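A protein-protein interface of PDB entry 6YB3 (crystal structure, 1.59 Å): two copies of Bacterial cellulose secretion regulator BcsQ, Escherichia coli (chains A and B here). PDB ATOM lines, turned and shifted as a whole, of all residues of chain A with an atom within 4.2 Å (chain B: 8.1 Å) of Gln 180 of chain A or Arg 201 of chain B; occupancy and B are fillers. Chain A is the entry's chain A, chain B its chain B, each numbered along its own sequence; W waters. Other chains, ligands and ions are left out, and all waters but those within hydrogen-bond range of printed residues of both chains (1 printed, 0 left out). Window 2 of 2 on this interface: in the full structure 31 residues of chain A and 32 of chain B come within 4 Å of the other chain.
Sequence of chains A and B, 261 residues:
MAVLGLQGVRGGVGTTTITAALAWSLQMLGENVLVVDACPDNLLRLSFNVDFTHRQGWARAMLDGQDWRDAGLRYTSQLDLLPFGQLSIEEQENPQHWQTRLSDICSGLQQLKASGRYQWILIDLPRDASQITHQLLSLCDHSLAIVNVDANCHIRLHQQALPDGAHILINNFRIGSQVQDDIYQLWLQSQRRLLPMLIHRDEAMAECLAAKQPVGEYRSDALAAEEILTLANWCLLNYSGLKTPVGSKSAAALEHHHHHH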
ATOM      1  N   VAL A 149     -27.186 -10.375 -35.284  1.00  0.00           N
ATOM      2  CA  VAL A 149     -28.477 -10.109 -34.662  1.00  0.00           C
ATOM      3  C   VAL A 149     -28.254  -9.360 -33.353  1.00  0.00           C
ATOM      4  O   VAL A 149     -28.004  -9.975 -32.307  1.00  0.00           O
ATOM      5  CB  VAL A 149     -29.284 -11.393 -34.408  1.00  0.00           C
ATOM      6  CG1 VAL A 149     -30.665 -11.025 -33.900  1.00  0.00           C
ATOM      7  CG2 VAL A 149     -29.371 -12.268 -35.672  1.00  0.00           C
ATOM      8  N   SER A 177     -29.724 -15.875 -26.062  1.00  0.00           N
ATOM      9  CA  SER A 177     -29.866 -14.482 -25.658  1.00  0.00           C
ATOM     10  C   SER A 177     -31.305 -14.057 -25.917  1.00  0.00           C
ATOM     11  O   SER A 177     -31.785 -14.155 -27.054  1.00  0.00           O
ATOM     12  CB  SER A 177     -28.885 -13.598 -26.424  1.00  0.00           C
ATOM     13  OG  SER A 177     -29.110 -12.220 -26.164  1.00  0.00           O
ATOM     14  N   GLN A 178     -31.999 -13.613 -24.863  1.00  0.00           N
ATOM     15  CA  GLN A 178     -33.408 -13.255 -25.002  1.00  0.00           C
ATOM     16  C   GLN A 178     -33.592 -12.115 -25.998  1.00  0.00           C
ATOM     17  O   GLN A 178     -34.417 -12.202 -26.917  1.00  0.00           O
ATOM     18  CB  GLN A 178     -33.997 -12.874 -23.650  1.00  0.00           C
ATOM     19  CG  GLN A 178     -35.411 -12.330 -23.743  1.00  0.00           C
ATOM     20  CD  GLN A 178     -36.428 -13.397 -24.095  1.00  0.00           C
ATOM     21  OE1 GLN A 178     -37.034 -13.364 -25.165  1.00  0.00           O
ATOM     22  NE2 GLN A 178     -36.632 -14.343 -23.185  1.00  0.00           N
ATOM     23  N   VAL A 179     -32.822 -11.040 -25.841  1.00  0.00           N
ATOM     24  CA  VAL A 179     -32.993  -9.901 -26.735  1.00  0.00           C
ATOM     25  C   VAL A 179     -32.596 -10.270 -28.158  1.00  0.00           C
ATOM     26  O   VAL A 179     -33.234  -9.833 -29.123  1.00  0.00           O
ATOM     27  CB  VAL A 179     -32.216  -8.673 -26.217  1.00  0.00           C
ATOM     28  CG1 VAL A 179     -30.703  -8.907 -26.264  1.00  0.00           C
ATOM     29  CG2 VAL A 179     -32.613  -7.434 -27.002  1.00  0.00           C
ATOM     30  N   GLN A 180     -31.567 -11.106 -28.320  1.00  0.00           N
ATOM     31  CA  GLN A 180     -31.170 -11.473 -29.676  1.00  0.00           C
ATOM     32  C   GLN A 180     -32.211 -12.372 -30.315  1.00  0.00           C
ATOM     33  O   GLN A 180     -32.528 -12.217 -31.501  1.00  0.00           O
ATOM     34  CB  GLN A 180     -29.781 -12.112 -29.658  1.00  0.00           C
ATOM     35  CG  GLN A 180     -28.729 -11.069 -29.263  1.00  0.00           C
ATOM     36  CD  GLN A 180     -27.340 -11.629 -29.078  1.00  0.00           C
ATOM     37  OE1 GLN A 180     -27.082 -12.799 -29.347  1.00  0.00           O
ATOM     38  NE2 GLN A 180     -26.432 -10.784 -28.614  1.00  0.00           N
ATOM     39  N   ASP A 181     -32.798 -13.282 -29.533  1.00  0.00           N
ATOM     40  CA  ASP A 181     -33.871 -14.118 -30.066  1.00  0.00           C
ATOM     41  C   ASP A 181     -35.105 -13.288 -30.399  1.00  0.00           C
ATOM     42  O   ASP A 181     -35.814 -13.604 -31.360  1.00  0.00           O
ATOM     43  CB  ASP A 181     -34.227 -15.234 -29.077  1.00  0.00           C
ATOM     44  CG  ASP A 181     -33.056 -16.182 -28.799  1.00  0.00           C
ATOM     45  OD1 ASP A 181     -32.145 -16.293 -29.646  1.00  0.00           O
ATOM     46  OD2 ASP A 181     -33.040 -16.805 -27.713  1.00  0.00           O
ATOM     47  N   ASP A 182     -35.380 -12.232 -29.626  1.00  0.00           N
ATOM     48  CA  ASP A 182     -36.510 -11.357 -29.933  1.00  0.00           C
ATOM     49  C   ASP A 182     -36.285 -10.611 -31.244  1.00  0.00           C
ATOM     50  O   ASP A 182     -37.177 -10.547 -32.098  1.00  0.00           O
ATOM     51  CB  ASP A 182     -36.740 -10.359 -28.796  1.00  0.00           C
ATOM     52  CG  ASP A 182     -37.298 -11.009 -27.548  1.00  0.00           C
ATOM     53  OD1 ASP A 182     -37.876 -12.109 -27.651  1.00  0.00           O
ATOM     54  OD2 ASP A 182     -37.160 -10.409 -26.463  1.00  0.00           O
ATOM     55  N   ILE A 183     -35.099 -10.027 -31.413  1.00  0.00           N
ATOM     56  CA  ILE A 183     -34.779  -9.344 -32.663  1.00  0.00           C
ATOM     57  C   ILE A 183     -34.877 -10.314 -33.836  1.00  0.00           C
ATOM     58  O   ILE A 183     -35.444  -9.991 -34.888  1.00  0.00           O
ATOM     59  CB  ILE A 183     -33.383  -8.698 -32.567  1.00  0.00           C
ATOM     60  CG1 ILE A 183     -33.381  -7.602 -31.495  1.00  0.00           C
ATOM     61  CG2 ILE A 183     -32.940  -8.142 -33.934  1.00  0.00           C
ATOM     62  CD1 ILE A 183     -32.020  -7.030 -31.192  1.00  0.00           C
ATOM     63  N   TYR A 184     -34.355 -11.527 -33.660  1.00  0.00           N
ATOM     64  CA  TYR A 184     -34.334 -12.497 -34.755  1.00  0.00           C
ATOM     65  C   TYR A 184     -35.747 -12.900 -35.174  1.00  0.00           C
ATOM     66  O   TYR A 184     -36.075 -12.903 -36.368  1.00  0.00           O
ATOM     67  CB  TYR A 184     -33.511 -13.714 -34.339  1.00  0.00           C
ATOM     68  CG  TYR A 184     -33.575 -14.876 -35.303  1.00  0.00           C
ATOM     69  CD1 TYR A 184     -32.984 -14.795 -36.552  1.00  0.00           C
ATOM     70  CD2 TYR A 184     -34.214 -16.059 -34.951  1.00  0.00           C
ATOM     71  CE1 TYR A 184     -33.033 -15.864 -37.437  1.00  0.00           C
ATOM     72  CE2 TYR A 184     -34.269 -17.128 -35.823  1.00  0.00           C
ATOM     73  CZ  TYR A 184     -33.679 -17.026 -37.064  1.00  0.00           C
ATOM     74  OH  TYR A 184     -33.736 -18.093 -37.930  1.00  0.00           O
ATOM     75  N   ARG A 201     -22.449 -18.600 -34.776  1.00  0.00           N
ATOM     76  CA  ARG A 201     -21.187 -18.466 -34.062  1.00  0.00           C
ATOM     77  C   ARG A 201     -20.525 -19.838 -33.982  1.00  0.00           C
ATOM     78  O   ARG A 201     -21.167 -20.835 -33.634  1.00  0.00           O
ATOM     79  CB  ARG A 201     -21.417 -17.884 -32.657  1.00  0.00           C
ATOM     80  CG  ARG A 201     -20.327 -18.239 -31.663  1.00  0.00           C
ATOM     81  CD  ARG A 201     -19.994 -17.081 -30.736  1.00  0.00           C
ATOM     82  NE  ARG A 201     -18.993 -16.217 -31.349  1.00  0.00           N
ATOM     83  CZ  ARG A 201     -18.655 -15.012 -30.903  1.00  0.00           C
ATOM     84  NH1 ARG A 201     -19.243 -14.503 -29.825  1.00  0.00           N
ATOM     85  NH2 ARG A 201     -17.727 -14.312 -31.546  1.00  0.00           N
ATOM     86  N   ILE B 170     -10.350  -3.942 -23.479  1.00  0.00           N
ATOM     87  CA  ILE B 170     -11.035  -5.137 -23.975  1.00  0.00           C
ATOM     88  C   ILE B 170     -12.520  -5.065 -23.626  1.00  0.00           C
ATOM     89  O   ILE B 170     -12.889  -4.776 -22.477  1.00  0.00           O
ATOM     90  CB  ILE B 170     -10.404  -6.406 -23.370  1.00  0.00           C
ATOM     91  CG1 ILE B 170      -8.973  -6.644 -23.875  1.00  0.00           C
ATOM     92  CG2 ILE B 170     -11.315  -7.635 -23.578  1.00  0.00           C
ATOM     93  CD1 ILE B 170      -8.180  -7.700 -23.054  1.00  0.00           C
ATOM     94  N   ASN B 171     -13.371  -5.341 -24.607  1.00  0.00           N
ATOM     95  CA  ASN B 171     -14.799  -5.599 -24.443  1.00  0.00           C
ATOM     96  C   ASN B 171     -15.125  -6.979 -25.024  1.00  0.00           C
ATOM     97  O   ASN B 171     -14.327  -7.562 -25.761  1.00  0.00           O
ATOM     98  CB  ASN B 171     -15.634  -4.514 -25.142  1.00  0.00           C
ATOM     99  CG  ASN B 171     -17.131  -4.651 -24.892  1.00  0.00           C
ATOM    100  OD1 ASN B 171     -17.574  -4.985 -23.790  1.00  0.00           O
ATOM    101  ND2 ASN B 171     -17.922  -4.408 -25.930  1.00  0.00           N
ATOM    102  N   ASN B 172     -16.312  -7.499 -24.688  1.00  0.00           N
ATOM    103  CA  ASN B 172     -16.863  -8.736 -25.240  1.00  0.00           C
ATOM    104  C   ASN B 172     -16.089  -9.997 -24.868  1.00  0.00           C
ATOM    105  O   ASN B 172     -16.186 -11.015 -25.578  1.00  0.00           O
ATOM    106  CB  ASN B 172     -16.977  -8.647 -26.781  1.00  0.00           C
ATOM    107  CG  ASN B 172     -18.216  -7.925 -27.219  1.00  0.00           C
ATOM    108  OD1 ASN B 172     -19.238  -7.972 -26.538  1.00  0.00           O
ATOM    109  ND2 ASN B 172     -18.146  -7.252 -28.373  1.00  0.00           N
ATOM    110  N   PHE B 173     -15.340 -10.000 -23.766  1.00  0.00           N
ATOM    111  CA  PHE B 173     -14.579 -11.191 -23.416  1.00  0.00           C
ATOM    112  C   PHE B 173     -15.553 -12.321 -23.091  1.00  0.00           C
ATOM    113  O   PHE B 173     -16.526 -12.105 -22.363  1.00  0.00           O
ATOM    114  CB  PHE B 173     -13.673 -10.877 -22.217  1.00  0.00           C
ATOM    115  CG  PHE B 173     -12.510 -11.827 -22.070  1.00  0.00           C
ATOM    116  CD1 PHE B 173     -11.377 -11.678 -22.859  1.00  0.00           C
ATOM    117  CD2 PHE B 173     -12.542 -12.847 -21.139  1.00  0.00           C
ATOM    118  CE1 PHE B 173     -10.306 -12.534 -22.726  1.00  0.00           C
ATOM    119  CE2 PHE B 173     -11.470 -13.702 -21.003  1.00  0.00           C
ATOM    120  CZ  PHE B 173     -10.346 -13.538 -21.790  1.00  0.00           C
ATOM    121  N   ARG B 174     -15.338 -13.519 -23.647  1.00  0.00           N
ATOM    122  CA  ARG B 174     -16.325 -14.568 -23.427  1.00  0.00           C
ATOM    123  C   ARG B 174     -15.701 -15.875 -22.955  1.00  0.00           C
ATOM    124  O   ARG B 174     -14.483 -16.078 -22.995  1.00  0.00           O
ATOM    125  CB  ARG B 174     -17.164 -14.826 -24.681  1.00  0.00           C
ATOM    126  CG  ARG B 174     -16.381 -15.171 -25.910  1.00  0.00           C
ATOM    127  CD  ARG B 174     -17.354 -15.271 -27.088  1.00  0.00           C
ATOM    128  NE  ARG B 174     -16.689 -15.491 -28.366  1.00  0.00           N
ATOM    129  CZ  ARG B 174     -16.295 -16.680 -28.806  1.00  0.00           C
ATOM    130  NH1 ARG B 174     -16.490 -17.760 -28.059  1.00  0.00           N
ATOM    131  NH2 ARG B 174     -15.703 -16.789 -29.993  1.00  0.00           N
ATOM    132  N   ILE B 175     -16.581 -16.750 -22.478  1.00  0.00           N
ATOM    133  CA  ILE B 175     -16.235 -18.134 -22.191  1.00  0.00           C
ATOM    134  C   ILE B 175     -16.336 -18.927 -23.487  1.00  0.00           C
ATOM    135  O   ILE B 175     -17.123 -18.589 -24.379  1.00  0.00           O
ATOM    136  CB  ILE B 175     -17.162 -18.724 -21.109  1.00  0.00           C
ATOM    137  CG1 ILE B 175     -17.189 -17.838 -19.867  1.00  0.00           C
ATOM    138  CG2 ILE B 175     -16.743 -20.172 -20.752  1.00  0.00           C
ATOM    139  CD1 ILE B 175     -15.824 -17.602 -19.245  1.00  0.00           C
ATOM    140  N   GLN B 180      -9.236 -17.106 -28.318  1.00  0.00           N
ATOM    141  CA  GLN B 180      -9.301 -15.874 -27.523  1.00  0.00           C
ATOM    142  C   GLN B 180      -8.398 -15.970 -26.303  1.00  0.00           C
ATOM    143  O   GLN B 180      -7.597 -15.066 -26.039  1.00  0.00           O
ATOM    144  CB  GLN B 180     -10.734 -15.588 -27.078  1.00  0.00           C
ATOM    145  CG  GLN B 180     -10.859 -14.400 -26.117  1.00  0.00           C
ATOM    146  CD  GLN B 180     -12.107 -14.513 -25.266  1.00  0.00           C
ATOM    147  OE1 GLN B 180     -13.107 -13.837 -25.524  1.00  0.00           O
ATOM    148  NE2 GLN B 180     -12.062 -15.386 -24.252  1.00  0.00           N
ATOM    149  N   LEU B 198     -11.126  -5.449 -17.830  1.00  0.00           N
ATOM    150  CA  LEU B 198     -11.801  -5.677 -19.105  1.00  0.00           C
ATOM    151  C   LEU B 198     -13.303  -5.775 -18.885  1.00  0.00           C
ATOM    152  O   LEU B 198     -13.791  -5.786 -17.750  1.00  0.00           O
ATOM    153  CB  LEU B 198     -11.252  -6.922 -19.796  1.00  0.00           C
ATOM    154  CG  LEU B 198     -11.209  -8.247 -19.031  1.00  0.00           C
ATOM    155  CD1 LEU B 198     -12.586  -8.882 -18.863  1.00  0.00           C
ATOM    156  CD2 LEU B 198     -10.259  -9.215 -19.740  1.00  0.00           C
ATOM    157  N   ILE B 199     -14.044  -5.843 -19.990  1.00  0.00           N
ATOM    158  CA  ILE B 199     -15.493  -5.984 -19.959  1.00  0.00           C
ATOM    159  C   ILE B 199     -15.847  -7.301 -20.635  1.00  0.00           C
ATOM    160  O   ILE B 199     -15.388  -7.569 -21.756  1.00  0.00           O
ATOM    161  CB  ILE B 199     -16.204  -4.812 -20.662  1.00  0.00           C
ATOM    162  CG1 ILE B 199     -15.694  -3.474 -20.130  1.00  0.00           C
ATOM    163  CG2 ILE B 199     -17.730  -4.943 -20.529  1.00  0.00           C
ATOM    164  CD1 ILE B 199     -15.917  -2.326 -21.063  1.00  0.00           C
ATOM    165  N   HIS B 200     -16.668  -8.118 -19.969  1.00  0.00           N
ATOM    166  CA  HIS B 200     -17.118  -9.379 -20.557  1.00  0.00           C
ATOM    167  C   HIS B 200     -18.315  -9.159 -21.472  1.00  0.00           C
ATOM    168  O   HIS B 200     -19.074  -8.194 -21.317  1.00  0.00           O
ATOM    169  CB  HIS B 200     -17.539 -10.389 -19.477  1.00  0.00           C
ATOM    170  CG  HIS B 200     -16.404 -11.087 -18.795  1.00  0.00           C
ATOM    171  ND1 HIS B 200     -15.693 -10.512 -17.763  1.00  0.00           N
ATOM    172  CD2 HIS B 200     -15.893 -12.330 -18.958  1.00  0.00           C
ATOM    173  CE1 HIS B 200     -14.774 -11.364 -17.338  1.00  0.00           C
ATOM    174  NE2 HIS B 200     -14.876 -12.476 -18.043  1.00  0.00           N
ATOM    175  N   ARG B 201     -18.485 -10.072 -22.433  1.00  0.00           N
ATOM    176  CA  ARG B 201     -19.793 -10.243 -23.049  1.00  0.00           C
ATOM    177  C   ARG B 201     -20.821 -10.521 -21.954  1.00  0.00           C
ATOM    178  O   ARG B 201     -20.635 -11.410 -21.114  1.00  0.00           O
ATOM    179  CB  ARG B 201     -19.782 -11.384 -24.085  1.00  0.00           C
ATOM    180  CG  ARG B 201     -21.114 -11.451 -24.863  1.00  0.00           C
ATOM    181  CD  ARG B 201     -21.195 -12.559 -25.902  1.00  0.00           C
ATOM    182  NE  ARG B 201     -22.482 -12.524 -26.603  1.00  0.00           N
ATOM    183  CZ  ARG B 201     -22.827 -13.344 -27.594  1.00  0.00           C
ATOM    184  NH1 ARG B 201     -21.981 -14.276 -28.014  1.00  0.00           N
ATOM    185  NH2 ARG B 201     -24.021 -13.231 -28.169  1.00  0.00           N
ATOM    186  N   ASP B 202     -21.911  -9.759 -21.972  1.00  0.00           N
ATOM    187  CA  ASP B 202     -22.866  -9.692 -20.881  1.00  0.00           C
ATOM    188  C   ASP B 202     -24.214  -9.315 -21.482  1.00  0.00           C
ATOM    189  O   ASP B 202     -24.311  -8.308 -22.201  1.00  0.00           O
ATOM    190  CB  ASP B 202     -22.379  -8.652 -19.848  1.00  0.00           C
ATOM    191  CG  ASP B 202     -23.208  -8.624 -18.563  1.00  0.00           C
ATOM    192  OD1 ASP B 202     -24.459  -8.652 -18.626  1.00  0.00           O
ATOM    193  OD2 ASP B 202     -22.594  -8.531 -17.468  1.00  0.00           O
ATOM    194  N   GLU B 203     -25.242 -10.119 -21.186  1.00  0.00           N
ATOM    195  CA  GLU B 203     -26.583  -9.848 -21.705  1.00  0.00           C
ATOM    196  C   GLU B 203     -27.078  -8.442 -21.353  1.00  0.00           C
ATOM    197  O   GLU B 203     -27.881  -7.868 -22.100  1.00  0.00           O
ATOM    198  CB  GLU B 203     -27.571 -10.895 -21.188  1.00  0.00           C
ATOM    199  CG  GLU B 203     -27.387 -12.280 -21.808  1.00  0.00           C
ATOM    200  CD  GLU B 203     -27.537 -12.270 -23.326  1.00  0.00           C
ATOM    201  OE1 GLU B 203     -28.506 -11.670 -23.836  1.00  0.00           O
ATOM    202  OE2 GLU B 203     -26.677 -12.866 -24.006  1.00  0.00           O
ATOM    203  N   ALA B 204     -26.628  -7.862 -20.236  1.00  0.00           N
ATOM    204  CA  ALA B 204     -27.063  -6.504 -19.910  1.00  0.00           C
ATOM    205  C   ALA B 204     -26.584  -5.494 -20.955  1.00  0.00           C
ATOM    206  O   ALA B 204     -27.266  -4.493 -21.227  1.00  0.00           O
ATOM    207  CB  ALA B 204     -26.564  -6.108 -18.516  1.00  0.00           C
ATOM    208  N   MET B 205     -25.389  -5.713 -21.509  1.00  0.00           N
ATOM    209  CA  MET B 205     -24.831  -4.833 -22.530  1.00  0.00           C
ATOM    210  C   MET B 205     -25.516  -5.025 -23.872  1.00  0.00           C
ATOM    211  O   MET B 205     -25.462  -4.124 -24.721  1.00  0.00           O
ATOM    212  CB  MET B 205     -23.328  -5.091 -22.678  1.00  0.00           C
ATOM    213  CG  MET B 205     -22.498  -4.693 -21.432  1.00  0.00           C
ATOM    214  SD  MET B 205     -22.144  -2.922 -21.352  1.00  0.00           S
ATOM    215  CE  MET B 205     -20.920  -2.775 -22.680  1.00  0.00           C
ATOM    216  N   ALA B 206     -26.145  -6.182 -24.083  1.00  0.00           N
ATOM    217  CA  ALA B 206     -26.924  -6.375 -25.298  1.00  0.00           C
ATOM    218  C   ALA B 206     -28.336  -5.840 -25.143  1.00  0.00           C
ATOM    219  O   ALA B 206     -28.910  -5.301 -26.105  1.00  0.00           O
ATOM    220  CB  ALA B 206     -26.957  -7.863 -25.679  1.00  0.00           C
ATOM    221  N   GLU B 207     -28.887  -5.932 -23.934  1.00  0.00           N
ATOM    222  CA  GLU B 207     -30.256  -5.506 -23.679  1.00  0.00           C
ATOM    223  C   GLU B 207     -30.376  -4.002 -23.479  1.00  0.00           C
ATOM    224  O   GLU B 207     -31.420  -3.426 -23.799  1.00  0.00           O
ATOM    225  CB  GLU B 207     -30.809  -6.214 -22.440  1.00  0.00           C
ATOM    226  CG  GLU B 207     -30.995  -7.713 -22.635  1.00  0.00           C
ATOM    227  CD  GLU B 207     -31.332  -8.445 -21.360  1.00  0.00           C
ATOM    228  OE1 GLU B 207     -31.477  -7.796 -20.314  1.00  0.00           O
ATOM    229  OE2 GLU B 207     -31.447  -9.682 -21.407  1.00  0.00           O
ATOM    230  N   ALA B 210     -31.439  -1.925 -26.377  1.00  0.00           N
ATOM    231  CA  ALA B 210     -32.833  -2.189 -26.711  1.00  0.00           C
ATOM    232  C   ALA B 210     -33.787  -1.546 -25.716  1.00  0.00           C
ATOM    233  O   ALA B 210     -34.941  -1.265 -26.065  1.00  0.00           O
ATOM    234  CB  ALA B 210     -33.080  -3.697 -26.787  1.00  0.00           C
ATOM    235  N   LEU B 223     -22.972  -7.506 -13.922  1.00  0.00           N
ATOM    236  CA  LEU B 223     -21.520  -7.657 -13.866  1.00  0.00           C
ATOM    237  C   LEU B 223     -20.821  -6.651 -14.785  1.00  0.00           C
ATOM    238  O   LEU B 223     -19.805  -6.054 -14.405  1.00  0.00           O
ATOM    239  CB  LEU B 223     -21.133  -9.103 -14.212  1.00  0.00           C
ATOM    240  CG  LEU B 223     -21.608 -10.100 -13.146  1.00  0.00           C
ATOM    241  CD1 LEU B 223     -21.329 -11.530 -13.583  1.00  0.00           C
ATOM    242  CD2 LEU B 223     -20.979  -9.801 -11.778  1.00  0.00           C
ATOM    243  N   ALA B 224     -21.376  -6.407 -15.981  1.00  0.00           N
ATOM    244  CA  ALA B 224     -20.761  -5.434 -16.881  1.00  0.00           C
ATOM    245  C   ALA B 224     -20.827  -4.014 -16.314  1.00  0.00           C
ATOM    246  O   ALA B 224     -19.897  -3.222 -16.515  1.00  0.00           O
ATOM    247  CB  ALA B 224     -21.422  -5.515 -18.260  1.00  0.00           C
ATOM    248  N   GLU B 227     -17.962  -3.792 -14.061  1.00  0.00           N
ATOM    249  CA  GLU B 227     -16.717  -3.686 -14.811  1.00  0.00           C
ATOM    250  C   GLU B 227     -16.521  -2.270 -15.333  1.00  0.00           C
ATOM    251  O   GLU B 227     -15.397  -1.750 -15.337  1.00  0.00           O
ATOM    252  CB  GLU B 227     -16.710  -4.701 -15.962  1.00  0.00           C
ATOM    253  CG  GLU B 227     -16.673  -6.146 -15.414  1.00  0.00           C
ATOM    254  CD  GLU B 227     -16.754  -7.241 -16.477  1.00  0.00           C
ATOM    255  OE1 GLU B 227     -17.551  -7.136 -17.440  1.00  0.00           O
ATOM    256  OE2 GLU B 227     -16.038  -8.253 -16.312  1.00  0.00           O
HETATM  257  O   HOH W   1     -30.984 -11.022 -23.520  1.00  0.00           O
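The guanidinium group (NH1) of Arg 201 of chain A lies close to the guanidinium group (NE) of Arg 174 of chain B (3.1 Å).
The side-chain hydroxyl of Ser 177 of chain A lies within hydrogen-bond range of the side-chain carboxylate of Glu 203 of chain B (2.5 Å).
NH1 of Arg 201 of chain A lies close to NH1 of Arg 201 of chain B, 3.3 Å away.
NH2 of Arg 201 of chain B is in hydrogen-bond range of OE1 of Gln 180 of chain A (3.3 Å).
O of Arg 174 of chain B sits at hydrogen-bond distance from NE2 of Gln 180 of chain B, 2.8 Å away.
The side-chain hydroxyl of Ser 177 of chain A lies close to the backbone NH of Gln 180 of chain A (3.5 Å).
The backbone NH (N) of Arg 201 of chain B is in hydrogen-bond range of the backbone carbonyl oxygen (O) of Phe 173 of chain B (2.8 Å).
CG1 of Val 179 of chain A touches CB of Ala 206 of chain B, 3.9 Å away.
Glu 207 of chain B touches Val 179 of chain A.
Val 179 of chain A touches Ala 210 of chain B.
Printed residues of chain B within 4 Å of Ser 177 of chain A: Glu 203 (2.5 Å).
Of chain B, only Ala 206 (3.9 Å), Glu 207 (3.8 Å) and Ala 210 (3.8 Å) come within 4 Å of Val 179 of chain A.
Of chain B, only Arg 201 (3.3 Å) comes within 4 Å of Gln 180 of chain A.
Printed residues of chain B within 4 Å of Arg 201 of chain A: Arg 174 and Arg 201.
Arg 201 of chain B touches just these residues of chain A: Gln 180 and Arg 201.
Of the printed residues of chain A, Glu 203 of chain B touches Ser 177 (2.5 Å).
Of the printed residues of chain A, Ala 210 of chain B touches Val 179 (3.8 Å).
The nearest printed residue of chain A that does not touch Arg 201 of chain B is Ser 177 of chain A (5.2 Å).
The nearest printed residue of chain A that does not touch Glu 207 of chain B is Gln 178 of chain A (4.7 Å).
Printed residues of chain B that touch a printed residue of chain A: Arg 174, Arg 201, Glu 203, Ala 206, Glu 207 and Ala 210.
Hydrophobic or aromatic side chains of chain B within 4 Å of the printed part of chain A: Ala 206 and Ala 210.
Hydrophobic or aromatic side chains of chain A that line the printed part of chain B: Val 179.
Among the printed residues, no Asp or Glu carboxylate lies within 4 Å of a Lys or Arg side-chain nitrogen of the other chain.
Gln 180 of chain A touches Arg 201 of chain B, but with the chains exchanged Arg 201 of chain A does not touch Gln 180 of chain B (7.5 Å).
Arg 201 of chain A touches its own counterpart, Arg 201 of chain B.
Of the 7 pairs that touch across the chains among the printed residues, 1 has its exchanged pair printed and touching as well.
Water W1 lies within hydrogen-bond range of the side-chain carboxylate (OE2) of Glu 207 of chain B (2.5 Å), the side-chain carboxylate (OE1) of Glu 203 of chain B (2.6 Å), the backbone NH (N) of Val 179 of chain A (3.0 Å), the backbone NH (N) of Gln 178 of chain A (3.1 Å) and the side-chain hydroxyl (OG) of Ser 177 of chain A (3.5 Å).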
